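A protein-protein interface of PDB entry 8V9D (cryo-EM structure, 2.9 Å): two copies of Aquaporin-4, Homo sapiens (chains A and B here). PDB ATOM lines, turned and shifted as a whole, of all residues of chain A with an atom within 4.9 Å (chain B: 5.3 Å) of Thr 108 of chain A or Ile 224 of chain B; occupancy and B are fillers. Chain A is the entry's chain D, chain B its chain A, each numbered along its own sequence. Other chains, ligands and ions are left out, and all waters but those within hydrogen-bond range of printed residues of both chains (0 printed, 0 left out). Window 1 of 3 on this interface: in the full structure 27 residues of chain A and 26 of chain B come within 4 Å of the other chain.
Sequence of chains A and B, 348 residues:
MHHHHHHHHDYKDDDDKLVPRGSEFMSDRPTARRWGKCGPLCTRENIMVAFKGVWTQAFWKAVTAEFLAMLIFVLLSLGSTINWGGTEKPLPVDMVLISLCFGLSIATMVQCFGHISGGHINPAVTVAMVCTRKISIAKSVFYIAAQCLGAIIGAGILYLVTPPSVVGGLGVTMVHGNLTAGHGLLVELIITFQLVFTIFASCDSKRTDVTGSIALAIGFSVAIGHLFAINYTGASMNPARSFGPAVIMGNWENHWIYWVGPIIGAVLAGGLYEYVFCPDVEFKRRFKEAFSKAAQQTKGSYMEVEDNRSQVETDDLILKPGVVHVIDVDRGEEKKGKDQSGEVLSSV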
ATOM      1  N   LEU A  76      22.808  -8.419 -21.450  1.00  0.00           N
ATOM      2  CA  LEU A  76      23.714  -7.295 -21.659  1.00  0.00           C
ATOM      3  C   LEU A  76      22.951  -5.999 -21.899  1.00  0.00           C
ATOM      4  O   LEU A  76      23.335  -4.942 -21.386  1.00  0.00           O
ATOM      5  CB  LEU A  76      24.655  -7.589 -22.825  1.00  0.00           C
ATOM      6  CG  LEU A  76      25.842  -8.507 -22.531  1.00  0.00           C
ATOM      7  CD1 LEU A  76      25.391  -9.936 -22.318  1.00  0.00           C
ATOM      8  CD2 LEU A  76      26.847  -8.431 -23.662  1.00  0.00           C
ATOM      9  N   CYS A 101      24.269   0.030 -26.836  1.00  0.00           N
ATOM     10  CA  CYS A 101      24.320  -1.334 -26.322  1.00  0.00           C
ATOM     11  C   CYS A 101      23.213  -2.191 -26.921  1.00  0.00           C
ATOM     12  O   CYS A 101      23.446  -3.346 -27.291  1.00  0.00           O
ATOM     13  CB  CYS A 101      24.234  -1.325 -24.796  1.00  0.00           C
ATOM     14  SG  CYS A 101      24.523  -2.933 -24.027  1.00  0.00           S
ATOM     15  N   LEU A 104      24.183  -2.535 -30.812  1.00  0.00           N
ATOM     16  CA  LEU A 104      25.351  -3.377 -31.039  1.00  0.00           C
ATOM     17  C   LEU A 104      25.172  -4.793 -30.510  1.00  0.00           C
ATOM     18  O   LEU A 104      25.887  -5.695 -30.952  1.00  0.00           O
ATOM     19  CB  LEU A 104      26.594  -2.749 -30.405  1.00  0.00           C
ATOM     20  CG  LEU A 104      27.043  -1.391 -30.944  1.00  0.00           C
ATOM     21  CD1 LEU A 104      28.276  -0.906 -30.205  1.00  0.00           C
ATOM     22  CD2 LEU A 104      27.313  -1.480 -32.430  1.00  0.00           C
ATOM     23  N   SER A 105      24.250  -5.004 -29.569  1.00  0.00           N
ATOM     24  CA  SER A 105      23.947  -6.360 -29.122  1.00  0.00           C
ATOM     25  C   SER A 105      23.207  -7.140 -30.198  1.00  0.00           C
ATOM     26  O   SER A 105      23.424  -8.345 -30.359  1.00  0.00           O
ATOM     27  CB  SER A 105      23.130  -6.318 -27.833  1.00  0.00           C
ATOM     28  OG  SER A 105      23.908  -5.856 -26.747  1.00  0.00           O
ATOM     29  N   ILE A 106      22.318  -6.472 -30.935  1.00  0.00           N
ATOM     30  CA  ILE A 106      21.618  -7.124 -32.037  1.00  0.00           C
ATOM     31  C   ILE A 106      22.574  -7.400 -33.189  1.00  0.00           C
ATOM     32  O   ILE A 106      22.520  -8.462 -33.817  1.00  0.00           O
ATOM     33  CB  ILE A 106      20.419  -6.271 -32.486  1.00  0.00           C
ATOM     34  CG1 ILE A 106      19.300  -6.336 -31.449  1.00  0.00           C
ATOM     35  CG2 ILE A 106      19.910  -6.738 -33.833  1.00  0.00           C
ATOM     36  CD1 ILE A 106      18.758  -7.725 -31.235  1.00  0.00           C
ATOM     37  N   ALA A 107      23.458  -6.449 -33.490  1.00  0.00           N
ATOM     38  CA  ALA A 107      24.421  -6.655 -34.564  1.00  0.00           C
ATOM     39  C   ALA A 107      25.332  -7.839 -34.279  1.00  0.00           C
ATOM     40  O   ALA A 107      25.829  -8.478 -35.212  1.00  0.00           O
ATOM     41  CB  ALA A 107      25.248  -5.388 -34.776  1.00  0.00           C
ATOM     42  N   THR A 108      25.564  -8.146 -33.002  1.00  0.00           N
ATOM     43  CA  THR A 108      26.483  -9.219 -32.640  1.00  0.00           C
ATOM     44  C   THR A 108      25.815 -10.585 -32.707  1.00  0.00           C
ATOM     45  O   THR A 108      26.416 -11.546 -33.196  1.00  0.00           O
ATOM     46  CB  THR A 108      27.050  -8.971 -31.243  1.00  0.00           C
ATOM     47  OG1 THR A 108      27.706  -7.699 -31.213  1.00  0.00           O
ATOM     48  CG2 THR A 108      28.044 -10.052 -30.870  1.00  0.00           C
ATOM     49  N   MET A 109      24.575 -10.696 -32.225  1.00  0.00           N
ATOM     50  CA  MET A 109      23.882 -11.980 -32.266  1.00  0.00           C
ATOM     51  C   MET A 109      23.415 -12.330 -33.670  1.00  0.00           C
ATOM     52  O   MET A 109      23.238 -13.513 -33.980  1.00  0.00           O
ATOM     53  CB  MET A 109      22.708 -11.978 -31.290  1.00  0.00           C
ATOM     54  CG  MET A 109      23.074 -11.532 -29.890  1.00  0.00           C
ATOM     55  SD  MET A 109      24.185 -12.712 -29.100  1.00  0.00           S
ATOM     56  CE  MET A 109      25.251 -11.617 -28.172  1.00  0.00           C
ATOM     57  N   VAL A 110      23.192 -11.332 -34.524  1.00  0.00           N
ATOM     58  CA  VAL A 110      22.927 -11.614 -35.931  1.00  0.00           C
ATOM     59  C   VAL A 110      24.174 -12.177 -36.597  1.00  0.00           C
ATOM     60  O   VAL A 110      24.101 -13.118 -37.395  1.00  0.00           O
ATOM     61  CB  VAL A 110      22.423 -10.348 -36.645  1.00  0.00           C
ATOM     62  CG1 VAL A 110      22.250 -10.609 -38.129  1.00  0.00           C
ATOM     63  CG2 VAL A 110      21.121  -9.875 -36.033  1.00  0.00           C
ATOM     64  N   GLN A 111      25.338 -11.604 -36.286  1.00  0.00           N
ATOM     65  CA  GLN A 111      26.596 -12.136 -36.793  1.00  0.00           C
ATOM     66  C   GLN A 111      26.859 -13.540 -36.260  1.00  0.00           C
ATOM     67  O   GLN A 111      27.306 -14.421 -37.002  1.00  0.00           O
ATOM     68  CB  GLN A 111      27.740 -11.195 -36.414  1.00  0.00           C
ATOM     69  CG  GLN A 111      29.112 -11.636 -36.886  1.00  0.00           C
ATOM     70  CD  GLN A 111      29.378 -11.279 -38.332  1.00  0.00           C
ATOM     71  OE1 GLN A 111      28.533 -11.477 -39.200  1.00  0.00           O
ATOM     72  NE2 GLN A 111      30.563 -10.750 -38.598  1.00  0.00           N
ATOM     73  N   CYS A 112      26.594 -13.763 -34.972  1.00  0.00           N
ATOM     74  CA  CYS A 112      26.913 -15.045 -34.353  1.00  0.00           C
ATOM     75  C   CYS A 112      25.996 -16.153 -34.854  1.00  0.00           C
ATOM     76  O   CYS A 112      26.461 -17.228 -35.246  1.00  0.00           O
ATOM     77  CB  CYS A 112      26.815 -14.924 -32.833  1.00  0.00           C
ATOM     78  SG  CYS A 112      28.178 -14.060 -32.049  1.00  0.00           S
ATOM     79  N   GLN B 194      30.343 -14.771 -25.248  1.00  0.00           N
ATOM     80  CA  GLN B 194      29.856 -14.176 -26.485  1.00  0.00           C
ATOM     81  C   GLN B 194      30.964 -13.546 -27.315  1.00  0.00           C
ATOM     82  O   GLN B 194      30.783 -13.360 -28.522  1.00  0.00           O
ATOM     83  CB  GLN B 194      28.767 -13.146 -26.172  1.00  0.00           C
ATOM     84  CG  GLN B 194      29.204 -11.974 -25.307  1.00  0.00           C
ATOM     85  CD  GLN B 194      29.830 -10.847 -26.097  1.00  0.00           C
ATOM     86  OE1 GLN B 194      29.507 -10.636 -27.263  1.00  0.00           O
ATOM     87  NE2 GLN B 194      30.719 -10.101 -25.455  1.00  0.00           N
ATOM     88  N   THR B 198      31.756 -14.977 -31.205  1.00  0.00           N
ATOM     89  CA  THR B 198      31.843 -14.052 -32.332  1.00  0.00           C
ATOM     90  C   THR B 198      33.115 -14.271 -33.139  1.00  0.00           C
ATOM     91  O   THR B 198      33.092 -14.206 -34.373  1.00  0.00           O
ATOM     92  CB  THR B 198      31.777 -12.611 -31.829  1.00  0.00           C
ATOM     93  OG1 THR B 198      30.707 -12.485 -30.886  1.00  0.00           O
ATOM     94  CG2 THR B 198      31.552 -11.650 -32.979  1.00  0.00           C
ATOM     95  N   ALA B 217      33.637  -6.274 -36.471  1.00  0.00           N
ATOM     96  CA  ALA B 217      32.644  -7.111 -35.807  1.00  0.00           C
ATOM     97  C   ALA B 217      33.126  -7.554 -34.434  1.00  0.00           C
ATOM     98  O   ALA B 217      32.354  -7.562 -33.468  1.00  0.00           O
ATOM     99  CB  ALA B 217      32.317  -8.325 -36.673  1.00  0.00           C
ATOM    100  N   PHE B 220      33.109  -4.417 -31.863  1.00  0.00           N
ATOM    101  CA  PHE B 220      31.804  -4.124 -31.282  1.00  0.00           C
ATOM    102  C   PHE B 220      31.351  -5.186 -30.292  1.00  0.00           C
ATOM    103  O   PHE B 220      30.473  -4.910 -29.470  1.00  0.00           O
ATOM    104  CB  PHE B 220      30.761  -3.966 -32.385  1.00  0.00           C
ATOM    105  CG  PHE B 220      30.911  -2.707 -33.184  1.00  0.00           C
ATOM    106  CD1 PHE B 220      31.671  -1.655 -32.705  1.00  0.00           C
ATOM    107  CD2 PHE B 220      30.301  -2.577 -34.416  1.00  0.00           C
ATOM    108  CE1 PHE B 220      31.808  -0.495 -33.433  1.00  0.00           C
ATOM    109  CE2 PHE B 220      30.440  -1.420 -35.149  1.00  0.00           C
ATOM    110  CZ  PHE B 220      31.194  -0.378 -34.657  1.00  0.00           C
ATOM    111  N   SER B 221      31.912  -6.393 -30.358  1.00  0.00           N
ATOM    112  CA  SER B 221      31.603  -7.399 -29.348  1.00  0.00           C
ATOM    113  C   SER B 221      32.290  -7.075 -28.030  1.00  0.00           C
ATOM    114  O   SER B 221      31.736  -7.327 -26.954  1.00  0.00           O
ATOM    115  CB  SER B 221      32.014  -8.782 -29.842  1.00  0.00           C
ATOM    116  OG  SER B 221      31.628  -9.777 -28.916  1.00  0.00           O
ATOM    117  N   VAL B 222      33.501  -6.523 -28.095  1.00  0.00           N
ATOM    118  CA  VAL B 222      34.187  -6.080 -26.888  1.00  0.00           C
ATOM    119  C   VAL B 222      33.487  -4.867 -26.289  1.00  0.00           C
ATOM    120  O   VAL B 222      33.427  -4.709 -25.065  1.00  0.00           O
ATOM    121  CB  VAL B 222      35.666  -5.790 -27.199  1.00  0.00           C
ATOM    122  CG1 VAL B 222      36.328  -5.089 -26.030  1.00  0.00           C
ATOM    123  CG2 VAL B 222      36.394  -7.074 -27.537  1.00  0.00           C
ATOM    124  N   ALA B 223      32.955  -3.988 -27.139  1.00  0.00           N
ATOM    125  CA  ALA B 223      32.317  -2.770 -26.651  1.00  0.00           C
ATOM    126  C   ALA B 223      31.066  -3.075 -25.835  1.00  0.00           C
ATOM    127  O   ALA B 223      30.844  -2.464 -24.786  1.00  0.00           O
ATOM    128  CB  ALA B 223      31.980  -1.852 -27.823  1.00  0.00           C
ATOM    129  N   ILE B 224      30.229  -4.004 -26.303  1.00  0.00           N
ATOM    130  CA  ILE B 224      28.994  -4.304 -25.584  1.00  0.00           C
ATOM    131  C   ILE B 224      29.287  -4.971 -24.248  1.00  0.00           C
ATOM    132  O   ILE B 224      28.554  -4.772 -23.274  1.00  0.00           O
ATOM    133  CB  ILE B 224      28.049  -5.157 -26.449  1.00  0.00           C
ATOM    134  CG1 ILE B 224      28.629  -6.550 -26.681  1.00  0.00           C
ATOM    135  CG2 ILE B 224      27.768  -4.462 -27.764  1.00  0.00           C
ATOM    136  CD1 ILE B 224      27.730  -7.453 -27.485  1.00  0.00           C
ATOM    137  N   GLY B 225      30.345  -5.780 -24.174  1.00  0.00           N
ATOM    138  CA  GLY B 225      30.743  -6.335 -22.894  1.00  0.00           C
ATOM    139  C   GLY B 225      31.158  -5.273 -21.897  1.00  0.00           C
ATOM    140  O   GLY B 225      30.939  -5.425 -20.694  1.00  0.00           O
ATOM    141  N   HIS B 226      31.771  -4.191 -22.377  1.00  0.00           N
ATOM    142  CA  HIS B 226      32.145  -3.089 -21.499  1.00  0.00           C
ATOM    143  C   HIS B 226      30.943  -2.229 -21.129  1.00  0.00           C
ATOM    144  O   HIS B 226      30.846  -1.752 -19.996  1.00  0.00           O
ATOM    145  CB  HIS B 226      33.229  -2.237 -22.160  1.00  0.00           C
ATOM    146  CG  HIS B 226      34.614  -2.752 -21.939  1.00  0.00           C
ATOM    147  ND1 HIS B 226      35.142  -3.801 -22.659  1.00  0.00           N
ATOM    148  CD2 HIS B 226      35.578  -2.374 -21.067  1.00  0.00           C
ATOM    149  CE1 HIS B 226      36.372  -4.042 -22.244  1.00  0.00           C
ATOM    150  NE2 HIS B 226      36.659  -3.192 -21.278  1.00  0.00           N
ATOM    151  N   LEU B 227      30.015  -2.025 -22.063  1.00  0.00           N
ATOM    152  CA  LEU B 227      28.834  -1.224 -21.765  1.00  0.00           C
ATOM    153  C   LEU B 227      27.971  -1.863 -20.686  1.00  0.00           C
ATOM    154  O   LEU B 227      27.105  -1.190 -20.119  1.00  0.00           O
ATOM    155  CB  LEU B 227      28.008  -1.011 -23.033  1.00  0.00           C
ATOM    156  CG  LEU B 227      28.573  -0.031 -24.061  1.00  0.00           C
ATOM    157  CD1 LEU B 227      27.946  -0.265 -25.424  1.00  0.00           C
ATOM    158  CD2 LEU B 227      28.370   1.402 -23.613  1.00  0.00           C
ATOM    159  N   PHE B 228      28.187  -3.143 -20.396  1.00  0.00           N
ATOM    160  CA  PHE B 228      27.426  -3.886 -19.402  1.00  0.00           C
ATOM    161  C   PHE B 228      28.127  -3.980 -18.051  1.00  0.00           C
ATOM    162  O   PHE B 228      27.530  -3.647 -17.024  1.00  0.00           O
ATOM    163  CB  PHE B 228      27.131  -5.295 -19.931  1.00  0.00           C
ATOM    164  CG  PHE B 228      26.575  -6.232 -18.897  1.00  0.00           C
ATOM    165  CD1 PHE B 228      25.577  -5.828 -18.033  1.00  0.00           C
ATOM    166  CD2 PHE B 228      27.063  -7.520 -18.785  1.00  0.00           C
ATOM    167  CE1 PHE B 228      25.077  -6.690 -17.085  1.00  0.00           C
ATOM    168  CE2 PHE B 228      26.564  -8.382 -17.838  1.00  0.00           C
ATOM    169  CZ  PHE B 228      25.573  -7.967 -16.989  1.00  0.00           C
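SG of Cys 112 of chain A lies within hydrogen-bond range of OG1 of Thr 198 of chain B, at 3.2 Å.
The backbone carbonyl oxygen (O) of Thr 108 of chain A is in hydrogen-bond range of the side-chain sulfur (SG) of Cys 112 of chain A, 3.3 Å away.
The side-chain amide oxygen of Gln 194 of chain B sits at hydrogen-bond distance from the side-chain hydroxyl of Ser 221 of chain B, at 2.8 Å.
The backbone carbonyl oxygen (O) of Leu 104 of chain A sits at hydrogen-bond distance from the side-chain hydroxyl (OG1) of Thr 108 of chain A.
The backbone carbonyl oxygen of Gln 194 of chain B sits at hydrogen-bond distance from the side-chain hydroxyl of Thr 198 of chain B.
The backbone carbonyl oxygen of Cys 101 of chain A is in hydrogen-bond range of the side-chain hydroxyl of Ser 105 of chain A (2.6 Å).
OG1 of Thr 198 of chain B sits at hydrogen-bond distance from OG of Ser 221 of chain B, 3.5 Å away.
Among the printed residues, pairs that only touch across the chains: Leu 104 of chain A with Ile 224 of chain B (3.4 Å), Gln 111 of chain A with Ala 217 of chain B (3.6 Å), Thr 108 of chain A with Thr 198 of chain B (3.6 Å), Thr 108 of chain A with Ile 224 of chain B (3.7 Å), Leu 104 of chain A with Phe 220 of chain B (3.8 Å), Cys 101 of chain A with Leu 227 of chain B (3.9 Å), Thr 108 of chain A with Gln 194 of chain B (3.9 Å), Leu 76 of chain A with Ile 224 of chain B (3.98 Å) and Ser 105 of chain A with Ile 224 of chain B (3.99 Å).
Of chain B, only Gln 194 (3.9 Å), Thr 198 (3.6 Å) and Ile 224 (3.7 Å) come within 4 Å of Thr 108 of chain A.
Of the printed residues of chain A, Ile 224 of chain B touches Leu 76, Leu 104, Ser 105 and Thr 108.
Of the printed residues of chain B, Ser 105 of chain A touches Ile 224 (3.99 Å).
Printed residues of chain A within 4 Å of Thr 198 of chain B: Thr 108 (3.6 Å) and Cys 112 (3.2 Å).
The nearest residue of chain B that does not touch Thr 108 of chain A is Ser 221 of chain B (4.1 Å).
The nearest printed residue of chain A that does not touch Gln 194 of chain B is Met 109 of chain A (4.3 Å).
Of the 12 printed residues of chain B, 6 touch a printed residue of chain A.
Among the printed residues, 10 pairs touch across the chains.
No position is printed for both chains.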
